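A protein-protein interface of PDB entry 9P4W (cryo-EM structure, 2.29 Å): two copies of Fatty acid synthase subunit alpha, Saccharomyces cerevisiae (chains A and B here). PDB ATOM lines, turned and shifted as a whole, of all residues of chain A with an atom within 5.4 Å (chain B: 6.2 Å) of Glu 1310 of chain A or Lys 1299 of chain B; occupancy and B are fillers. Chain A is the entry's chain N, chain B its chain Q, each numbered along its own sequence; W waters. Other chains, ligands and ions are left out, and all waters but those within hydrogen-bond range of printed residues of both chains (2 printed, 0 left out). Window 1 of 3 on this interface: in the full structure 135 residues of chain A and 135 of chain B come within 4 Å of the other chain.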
ATOM      1  N   PRO A1301     -15.406   8.660 -20.371  1.00  0.00           N
ATOM      2  CA  PRO A1301     -16.117   7.922 -19.322  1.00  0.00           C
ATOM      3  C   PRO A1301     -15.172   7.094 -18.467  1.00  0.00           C
ATOM      4  O   PRO A1301     -14.081   6.707 -18.890  1.00  0.00           O
ATOM      5  CB  PRO A1301     -17.083   7.022 -20.102  1.00  0.00           C
ATOM      6  CG  PRO A1301     -16.600   7.007 -21.514  1.00  0.00           C
ATOM      7  CD  PRO A1301     -15.475   7.976 -21.672  1.00  0.00           C
ATOM      8  N   VAL A1302     -15.613   6.830 -17.242  1.00  0.00           N
ATOM      9  CA  VAL A1302     -14.942   5.920 -16.326  1.00  0.00           C
ATOM     10  C   VAL A1302     -16.022   5.004 -15.774  1.00  0.00           C
ATOM     11  O   VAL A1302     -16.868   5.441 -14.985  1.00  0.00           O
ATOM     12  CB  VAL A1302     -14.212   6.653 -15.192  1.00  0.00           C
ATOM     13  CG1 VAL A1302     -13.499   5.660 -14.291  1.00  0.00           C
ATOM     14  CG2 VAL A1302     -13.233   7.661 -15.761  1.00  0.00           C
ATOM     15  N   GLY A1303     -16.006   3.742 -16.192  1.00  0.00           N
ATOM     16  CA  GLY A1303     -17.064   2.825 -15.822  1.00  0.00           C
ATOM     17  C   GLY A1303     -16.583   1.446 -15.437  1.00  0.00           C
ATOM     18  O   GLY A1303     -17.319   0.467 -15.586  1.00  0.00           O
ATOM     19  N   ALA A1306     -17.593  -1.750 -17.421  1.00  0.00           N
ATOM     20  CA  ALA A1306     -18.611  -1.345 -18.383  1.00  0.00           C
ATOM     21  C   ALA A1306     -18.216  -0.071 -19.123  1.00  0.00           C
ATOM     22  O   ALA A1306     -19.078   0.609 -19.700  1.00  0.00           O
ATOM     23  CB  ALA A1306     -19.956  -1.158 -17.680  1.00  0.00           C
ATOM     24  N   THR A1307     -16.922   0.256 -19.112  1.00  0.00           N
ATOM     25  CA  THR A1307     -16.454   1.514 -19.677  1.00  0.00           C
ATOM     26  C   THR A1307     -16.772   1.618 -21.161  1.00  0.00           C
ATOM     27  O   THR A1307     -17.165   2.683 -21.642  1.00  0.00           O
ATOM     28  CB  THR A1307     -14.949   1.655 -19.452  1.00  0.00           C
ATOM     29  OG1 THR A1307     -14.629   1.311 -18.099  1.00  0.00           O
ATOM     30  CG2 THR A1307     -14.501   3.076 -19.730  1.00  0.00           C
ATOM     31  N   SER A1308     -16.596   0.528 -21.906  1.00  0.00           N
ATOM     32  CA  SER A1308     -16.771   0.596 -23.352  1.00  0.00           C
ATOM     33  C   SER A1308     -18.234   0.790 -23.728  1.00  0.00           C
ATOM     34  O   SER A1308     -18.549   1.573 -24.632  1.00  0.00           O
ATOM     35  CB  SER A1308     -16.211  -0.665 -24.001  1.00  0.00           C
ATOM     36  OG  SER A1308     -14.805  -0.724 -23.865  1.00  0.00           O
ATOM     37  N   VAL A1309     -19.144   0.086 -23.052  1.00  0.00           N
ATOM     38  CA  VAL A1309     -20.568   0.275 -23.317  1.00  0.00           C
ATOM     39  C   VAL A1309     -20.991   1.687 -22.929  1.00  0.00           C
ATOM     40  O   VAL A1309     -21.775   2.333 -23.639  1.00  0.00           O
ATOM     41  CB  VAL A1309     -21.397  -0.793 -22.581  1.00  0.00           C
ATOM     42  CG1 VAL A1309     -22.884  -0.539 -22.769  1.00  0.00           C
ATOM     43  CG2 VAL A1309     -21.031  -2.179 -23.076  1.00  0.00           C
ATOM     44  N   GLU A1310     -20.485   2.191 -21.802  1.00  0.00           N
ATOM     45  CA  GLU A1310     -20.788   3.567 -21.424  1.00  0.00           C
ATOM     46  C   GLU A1310     -20.267   4.548 -22.468  1.00  0.00           C
ATOM     47  O   GLU A1310     -20.925   5.547 -22.778  1.00  0.00           O
ATOM     48  CB  GLU A1310     -20.193   3.870 -20.049  1.00  0.00           C
ATOM     49  CG  GLU A1310     -20.278   5.327 -19.631  1.00  0.00           C
ATOM     50  CD  GLU A1310     -19.668   5.573 -18.267  1.00  0.00           C
ATOM     51  OE1 GLU A1310     -19.299   4.589 -17.595  1.00  0.00           O
ATOM     52  OE2 GLU A1310     -19.556   6.749 -17.868  1.00  0.00           O
ATOM     53  N   SER A1311     -19.081   4.280 -23.015  1.00  0.00           N
ATOM     54  CA  SER A1311     -18.521   5.128 -24.058  1.00  0.00           C
ATOM     55  C   SER A1311     -19.400   5.118 -25.301  1.00  0.00           C
ATOM     56  O   SER A1311     -19.633   6.163 -25.919  1.00  0.00           O
ATOM     57  CB  SER A1311     -17.103   4.664 -24.391  1.00  0.00           C
ATOM     58  OG  SER A1311     -16.678   5.153 -25.647  1.00  0.00           O
ATOM     59  N   VAL A1312     -19.896   3.941 -25.686  1.00  0.00           N
ATOM     60  CA  VAL A1312     -20.790   3.854 -26.838  1.00  0.00           C
ATOM     61  C   VAL A1312     -22.056   4.665 -26.587  1.00  0.00           C
ATOM     62  O   VAL A1312     -22.536   5.391 -27.465  1.00  0.00           O
ATOM     63  CB  VAL A1312     -21.117   2.385 -27.162  1.00  0.00           C
ATOM     64  CG1 VAL A1312     -22.197   2.306 -28.227  1.00  0.00           C
ATOM     65  CG2 VAL A1312     -19.872   1.651 -27.626  1.00  0.00           C
ATOM     66  N   ASP A1313     -22.625   4.540 -25.388  1.00  0.00           N
ATOM     67  CA  ASP A1313     -23.837   5.288 -25.061  1.00  0.00           C
ATOM     68  C   ASP A1313     -23.589   6.791 -25.147  1.00  0.00           C
ATOM     69  O   ASP A1313     -24.376   7.536 -25.750  1.00  0.00           O
ATOM     70  CB  ASP A1313     -24.319   4.892 -23.663  1.00  0.00           C
ATOM     71  CG  ASP A1313     -25.521   5.698 -23.197  1.00  0.00           C
ATOM     72  OD1 ASP A1313     -26.039   6.529 -23.969  1.00  0.00           O
ATOM     73  OD2 ASP A1313     -25.953   5.498 -22.044  1.00  0.00           O
ATOM     74  N   ILE A1314     -22.485   7.253 -24.554  1.00  0.00           N
ATOM     75  CA  ILE A1314     -22.172   8.679 -24.570  1.00  0.00           C
ATOM     76  C   ILE A1314     -21.947   9.160 -25.995  1.00  0.00           C
ATOM     77  O   ILE A1314     -22.375  10.254 -26.365  1.00  0.00           O
ATOM     78  CB  ILE A1314     -20.958   8.977 -23.672  1.00  0.00           C
ATOM     79  CG1 ILE A1314     -21.329   8.792 -22.201  1.00  0.00           C
ATOM     80  CG2 ILE A1314     -20.447  10.387 -23.911  1.00  0.00           C
ATOM     81  CD1 ILE A1314     -20.157   8.481 -21.316  1.00  0.00           C
ATOM     82  N   GLY A1315     -21.261   8.363 -26.815  1.00  0.00           N
ATOM     83  CA  GLY A1315     -21.025   8.772 -28.189  1.00  0.00           C
ATOM     84  C   GLY A1315     -22.302   8.857 -28.999  1.00  0.00           C
ATOM     85  O   GLY A1315     -22.492   9.787 -29.789  1.00  0.00           O
ATOM     86  N   GLU A1317     -25.293   9.490 -27.831  1.00  0.00           N
ATOM     87  CA  GLU A1317     -26.036  10.673 -27.404  1.00  0.00           C
ATOM     88  C   GLU A1317     -25.350  11.960 -27.847  1.00  0.00           C
ATOM     89  O   GLU A1317     -26.025  12.956 -28.122  1.00  0.00           O
ATOM     90  CB  GLU A1317     -26.221  10.664 -25.885  1.00  0.00           C
ATOM     91  CG  GLU A1317     -27.422   9.864 -25.351  1.00  0.00           C
ATOM     92  CD  GLU A1317     -28.542   9.659 -26.362  1.00  0.00           C
ATOM     93  OE1 GLU A1317     -29.013  10.657 -26.948  1.00  0.00           O
ATOM     94  OE2 GLU A1317     -28.948   8.498 -26.577  1.00  0.00           O
ATOM     95  N   THR A1409     -27.306   2.561 -19.909  1.00  0.00           N
ATOM     96  CA  THR A1409     -26.590   2.316 -18.665  1.00  0.00           C
ATOM     97  C   THR A1409     -27.573   2.403 -17.505  1.00  0.00           C
ATOM     98  O   THR A1409     -28.595   3.086 -17.593  1.00  0.00           O
ATOM     99  CB  THR A1409     -25.443   3.324 -18.451  1.00  0.00           C
ATOM    100  OG1 THR A1409     -25.975   4.646 -18.309  1.00  0.00           O
ATOM    101  CG2 THR A1409     -24.478   3.299 -19.625  1.00  0.00           C
ATOM    102  N   LYS A1649     -22.303  -0.486 -12.422  1.00  0.00           N
ATOM    103  CA  LYS A1649     -22.248  -0.006 -13.802  1.00  0.00           C
ATOM    104  C   LYS A1649     -22.739  -1.124 -14.716  1.00  0.00           C
ATOM    105  O   LYS A1649     -21.960  -1.940 -15.206  1.00  0.00           O
ATOM    106  CB  LYS A1649     -20.838   0.440 -14.165  1.00  0.00           C
ATOM    107  CG  LYS A1649     -20.453   1.783 -13.585  1.00  0.00           C
ATOM    108  CD  LYS A1649     -20.371   2.838 -14.669  1.00  0.00           C
ATOM    109  CE  LYS A1649     -19.929   4.178 -14.113  1.00  0.00           C
ATOM    110  NZ  LYS A1649     -19.768   5.194 -15.184  1.00  0.00           N
ATOM    111  N   ASN B1245     -26.934   9.980 -12.527  1.00  0.00           N
ATOM    112  CA  ASN B1245     -25.802  10.559 -11.815  1.00  0.00           C
ATOM    113  C   ASN B1245     -24.669  10.697 -12.820  1.00  0.00           C
ATOM    114  O   ASN B1245     -24.139   9.690 -13.297  1.00  0.00           O
ATOM    115  CB  ASN B1245     -25.384   9.698 -10.625  1.00  0.00           C
ATOM    116  CG  ASN B1245     -24.374  10.389  -9.733  1.00  0.00           C
ATOM    117  OD1 ASN B1245     -23.721  11.345 -10.141  1.00  0.00           O
ATOM    118  ND2 ASN B1245     -24.244   9.909  -8.505  1.00  0.00           N
ATOM    119  N   CYS B1246     -24.300  11.935 -13.143  1.00  0.00           N
ATOM    120  CA  CYS B1246     -23.334  12.208 -14.197  1.00  0.00           C
ATOM    121  C   CYS B1246     -22.164  13.049 -13.695  1.00  0.00           C
ATOM    122  O   CYS B1246     -21.530  13.762 -14.473  1.00  0.00           O
ATOM    123  CB  CYS B1246     -24.019  12.894 -15.378  1.00  0.00           C
ATOM    124  SG  CYS B1246     -25.117  11.810 -16.326  1.00  0.00           S
ATOM    125  N   SER B1247     -21.860  12.975 -12.402  1.00  0.00           N
ATOM    126  CA  SER B1247     -20.744  13.712 -11.831  1.00  0.00           C
ATOM    127  C   SER B1247     -19.481  12.854 -11.818  1.00  0.00           C
ATOM    128  O   SER B1247     -19.534  11.624 -11.863  1.00  0.00           O
ATOM    129  CB  SER B1247     -21.076  14.180 -10.413  1.00  0.00           C
ATOM    130  OG  SER B1247     -21.334  13.084  -9.560  1.00  0.00           O
ATOM    131  N   GLY B1248     -18.333  13.525 -11.764  1.00  0.00           N
ATOM    132  CA  GLY B1248     -17.061  12.829 -11.767  1.00  0.00           C
ATOM    133  C   GLY B1248     -15.942  13.592 -11.088  1.00  0.00           C
ATOM    134  O   GLY B1248     -16.183  14.609 -10.436  1.00  0.00           O
ATOM    135  N   PRO B1297     -29.379   6.202 -15.425  1.00  0.00           N
ATOM    136  CA  PRO B1297     -28.061   6.278 -16.067  1.00  0.00           C
ATOM    137  C   PRO B1297     -26.980   6.728 -15.094  1.00  0.00           C
ATOM    138  O   PRO B1297     -27.210   7.575 -14.227  1.00  0.00           O
ATOM    139  CB  PRO B1297     -28.264   7.295 -17.196  1.00  0.00           C
ATOM    140  CG  PRO B1297     -29.562   7.965 -16.930  1.00  0.00           C
ATOM    141  CD  PRO B1297     -30.371   7.098 -16.040  1.00  0.00           C
ATOM    142  N   ILE B1298     -25.791   6.154 -15.246  1.00  0.00           N
ATOM    143  CA  ILE B1298     -24.610   6.568 -14.502  1.00  0.00           C
ATOM    144  C   ILE B1298     -23.469   6.713 -15.500  1.00  0.00           C
ATOM    145  O   ILE B1298     -23.022   5.721 -16.089  1.00  0.00           O
ATOM    146  CB  ILE B1298     -24.244   5.587 -13.381  1.00  0.00           C
ATOM    147  CG1 ILE B1298     -22.922   6.005 -12.737  1.00  0.00           C
ATOM    148  CG2 ILE B1298     -24.176   4.153 -13.903  1.00  0.00           C
ATOM    149  CD1 ILE B1298     -22.912   5.857 -11.247  1.00  0.00           C
ATOM    150  N   LYS B1299     -23.003   7.941 -15.693  1.00  0.00           N
ATOM    151  CA  LYS B1299     -21.917   8.242 -16.619  1.00  0.00           C
ATOM    152  C   LYS B1299     -20.934   9.142 -15.888  1.00  0.00           C
ATOM    153  O   LYS B1299     -21.237  10.308 -15.625  1.00  0.00           O
ATOM    154  CB  LYS B1299     -22.443   8.915 -17.886  1.00  0.00           C
ATOM    155  CG  LYS B1299     -23.283   8.010 -18.764  1.00  0.00           C
ATOM    156  CD  LYS B1299     -24.474   8.751 -19.343  1.00  0.00           C
ATOM    157  CE  LYS B1299     -24.910   8.158 -20.667  1.00  0.00           C
ATOM    158  NZ  LYS B1299     -25.939   9.000 -21.332  1.00  0.00           N
ATOM    159  N   THR B1300     -19.760   8.607 -15.568  1.00  0.00           N
ATOM    160  CA  THR B1300     -18.810   9.324 -14.736  1.00  0.00           C
ATOM    161  C   THR B1300     -17.765   9.989 -15.619  1.00  0.00           C
ATOM    162  O   THR B1300     -16.924   9.284 -16.194  1.00  0.00           O
ATOM    163  CB  THR B1300     -18.144   8.373 -13.745  1.00  0.00           C
ATOM    164  OG1 THR B1300     -19.152   7.700 -12.983  1.00  0.00           O
ATOM    165  CG2 THR B1300     -17.241   9.135 -12.805  1.00  0.00           C
ATOM    166  N   PRO B1301     -17.768  11.311 -15.762  1.00  0.00           N
ATOM    167  CA  PRO B1301     -16.757  11.957 -16.603  1.00  0.00           C
ATOM    168  C   PRO B1301     -15.421  12.090 -15.890  1.00  0.00           C
ATOM    169  O   PRO B1301     -15.340  12.121 -14.661  1.00  0.00           O
ATOM    170  CB  PRO B1301     -17.359  13.335 -16.903  1.00  0.00           C
ATOM    171  CG  PRO B1301     -18.459  13.538 -15.916  1.00  0.00           C
ATOM    172  CD  PRO B1301     -18.664  12.288 -15.124  1.00  0.00           C
ATOM    173  N   ILE B1314     -22.856  16.424 -19.951  1.00  0.00           N
ATOM    174  CA  ILE B1314     -23.338  15.051 -20.051  1.00  0.00           C
ATOM    175  C   ILE B1314     -24.715  14.920 -19.419  1.00  0.00           C
ATOM    176  O   ILE B1314     -25.585  14.222 -19.942  1.00  0.00           O
ATOM    177  CB  ILE B1314     -22.329  14.076 -19.420  1.00  0.00           C
ATOM    178  CG1 ILE B1314     -21.067  13.990 -20.278  1.00  0.00           C
ATOM    179  CG2 ILE B1314     -22.946  12.698 -19.253  1.00  0.00           C
ATOM    180  CD1 ILE B1314     -19.844  13.571 -19.514  1.00  0.00           C
ATOM    181  N   GLU B1317     -27.383  16.424 -21.720  1.00  0.00           N
ATOM    182  CA  GLU B1317     -27.674  15.556 -22.859  1.00  0.00           C
ATOM    183  C   GLU B1317     -28.374  14.273 -22.425  1.00  0.00           C
ATOM    184  O   GLU B1317     -29.190  13.732 -23.177  1.00  0.00           O
ATOM    185  CB  GLU B1317     -26.387  15.229 -23.620  1.00  0.00           C
ATOM    186  CG  GLU B1317     -25.939  16.259 -24.671  1.00  0.00           C
ATOM    187  CD  GLU B1317     -27.058  17.145 -25.201  1.00  0.00           C
ATOM    188  OE1 GLU B1317     -28.092  16.606 -25.651  1.00  0.00           O
ATOM    189  OE2 GLU B1317     -26.908  18.383 -25.162  1.00  0.00           O
ATOM    190  N   THR B1318     -28.079  13.777 -21.223  1.00  0.00           N
ATOM    191  CA  THR B1318     -28.786  12.610 -20.707  1.00  0.00           C
ATOM    192  C   THR B1318     -30.260  12.915 -20.494  1.00  0.00           C
ATOM    193  O   THR B1318     -31.122  12.094 -20.825  1.00  0.00           O
ATOM    194  CB  THR B1318     -28.142  12.144 -19.398  1.00  0.00           C
ATOM    195  OG1 THR B1318     -26.761  11.844 -19.620  1.00  0.00           O
ATOM    196  CG2 THR B1318     -28.844  10.910 -18.854  1.00  0.00           C
ATOM    197  N   SER B1321     -31.955  13.360 -23.988  1.00  0.00           N
ATOM    198  CA  SER B1321     -32.142  12.125 -24.736  1.00  0.00           C
ATOM    199  C   SER B1321     -33.286  11.279 -24.197  1.00  0.00           C
ATOM    200  O   SER B1321     -33.649  10.285 -24.831  1.00  0.00           O
ATOM    201  CB  SER B1321     -30.853  11.299 -24.727  1.00  0.00           C
ATOM    202  OG  SER B1321     -30.663  10.660 -23.478  1.00  0.00           O
ATOM    203  N   LYS B1323     -33.196   9.609 -21.318  1.00  0.00           N
ATOM    204  CA  LYS B1323     -32.707   8.585 -20.406  1.00  0.00           C
ATOM    205  C   LYS B1323     -32.951   8.934 -18.948  1.00  0.00           C
ATOM    206  O   LYS B1323     -32.965   8.034 -18.103  1.00  0.00           O
ATOM    207  CB  LYS B1323     -31.210   8.357 -20.627  1.00  0.00           C
ATOM    208  CG  LYS B1323     -30.857   7.900 -22.029  1.00  0.00           C
ATOM    209  CD  LYS B1323     -31.314   6.471 -22.285  1.00  0.00           C
ATOM    210  CE  LYS B1323     -30.792   5.944 -23.615  1.00  0.00           C
ATOM    211  NZ  LYS B1323     -29.313   6.071 -23.740  1.00  0.00           N
HETATM  212  O   HOH W   1     -27.527   6.175 -26.403  1.00  0.00           O
HETATM  213  O   HOH W   2     -29.138  13.946 -26.605  1.00  0.00           O
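N of Val 1302 of chain A is in hydrogen-bond range of O of Thr 1300 of chain B.
The side-chain carboxylate (OE2) of Glu 1310 of chain A is in hydrogen-bond range of the backbone NH (N) of Thr 1300 of chain B (3.0 Å).
The side-chain carboxylate (OD2) of Asp 1313 of chain A lies within salt-bridge range of the side-chain amino group (NZ) of Lys 1299 of chain B (3.6 Å).
OD1 of Asp 1313 of chain A is in salt-bridge range of NZ of Lys 1323 of chain B, 3.3 Å away.
NZ of Lys 1323 of chain B is in salt-bridge range of OE2 of Glu 1317 of chain A (3.8 Å).
The side-chain hydroxyl (OG1) of Thr 1409 of chain A sits at hydrogen-bond distance from the backbone NH (N) of Ile 1298 of chain B (3.4 Å).
The side-chain amino group (NZ) of Lys 1649 of chain A is in hydrogen-bond range of the backbone carbonyl oxygen (O) of Ile 1298 of chain B, 3.4 Å away.
The side-chain amino group (NZ) of Lys 1649 of chain A lies within hydrogen-bond range of the side-chain hydroxyl (OG1) of Thr 1300 of chain B, 3.4 Å away.
The backbone carbonyl oxygen of Val 1302 of chain A sits at hydrogen-bond distance from the side-chain amino group of Lys 1649 of chain A (2.9 Å).
The side-chain amino group (NZ) of Lys 1299 of chain B lies within hydrogen-bond range of the side-chain hydroxyl (OG1) of Thr 1318 of chain B (3.4 Å).
The backbone carbonyl oxygen of Glu 1317 of chain B lies close to the side-chain hydroxyl of Ser 1321 of chain B.
The backbone carbonyl oxygen (O) of Thr 1318 of chain B is in hydrogen-bond range of the side-chain hydroxyl (OG) of Ser 1321 of chain B (3.1 Å).
The backbone carbonyl oxygen (O) of Thr 1318 of chain B sits at hydrogen-bond distance from the backbone NH (N) of Lys 1323 of chain B.
The backbone NH (N) of Lys 1323 of chain B sits close to the side-chain hydroxyl (OG) of Ser 1321 of chain B.
Pro 1301 of chain A touches Thr 1300 of chain B.
OE2 of Glu 1310 of chain A touches CA of Lys 1299 of chain B (3.1 Å).
Ile 1314 of chain A touches Lys 1299 of chain B (CG1 to CE, 3.9 Å).
Ser 1321 of chain B touches Glu 1317 of chain A (CB to OE1, 3.0 Å).
Thr 1409 of chain A touches Pro 1297 of chain B (OG1 to CA, 3.5 Å).
Lys 1299 of chain B touches Lys 1649 of chain A (CA to NZ, 3.996 Å).
Of the printed residues of chain A, Lys 1299 of chain B touches Glu 1310 (3.1 Å), Asp 1313 (3.2 Å), Ile 1314 (3.9 Å) and Lys 1649 (3.996 Å).
Of the printed residues of chain B, Lys 1649 of chain A touches Ile 1298, Lys 1299 and Thr 1300.
Of the printed residues of chain B, Glu 1317 of chain A touches Ser 1321 and Lys 1323.
Asn 1245 of chain B touches none of the printed residues of chain A.
Gly 1315 of chain A touches none of the printed residues of chain B.
Hydrophobic or aromatic side chains of chain A that line the printed part of chain B: Val 1302 and Ile 1314.
Among the printed residues, Asp or Glu carboxylates within 4 Å of a Lys or Arg side-chain nitrogen of the other chain: Asp 1313 of chain A with Lys 1299 of chain B (3.6 Å), Asp 1313 of chain A with Lys 1323 of chain B (3.3 Å) and Glu 1317 of chain A with Lys 1323 of chain B (3.8 Å).
Positions printed for both chains: 1301, 1314 and 1317.
Water W1 lies within hydrogen-bond range of OE2 of Glu 1317 of chain A (2.7 Å), OD1 of Asp 1313 of chain A (2.9 Å) and NZ of Lys 1323 of chain B (3.2 Å).
Water W2 bridges OE1 of Glu 1317 of chain B and OE1 of Glu 1317 of chain A.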
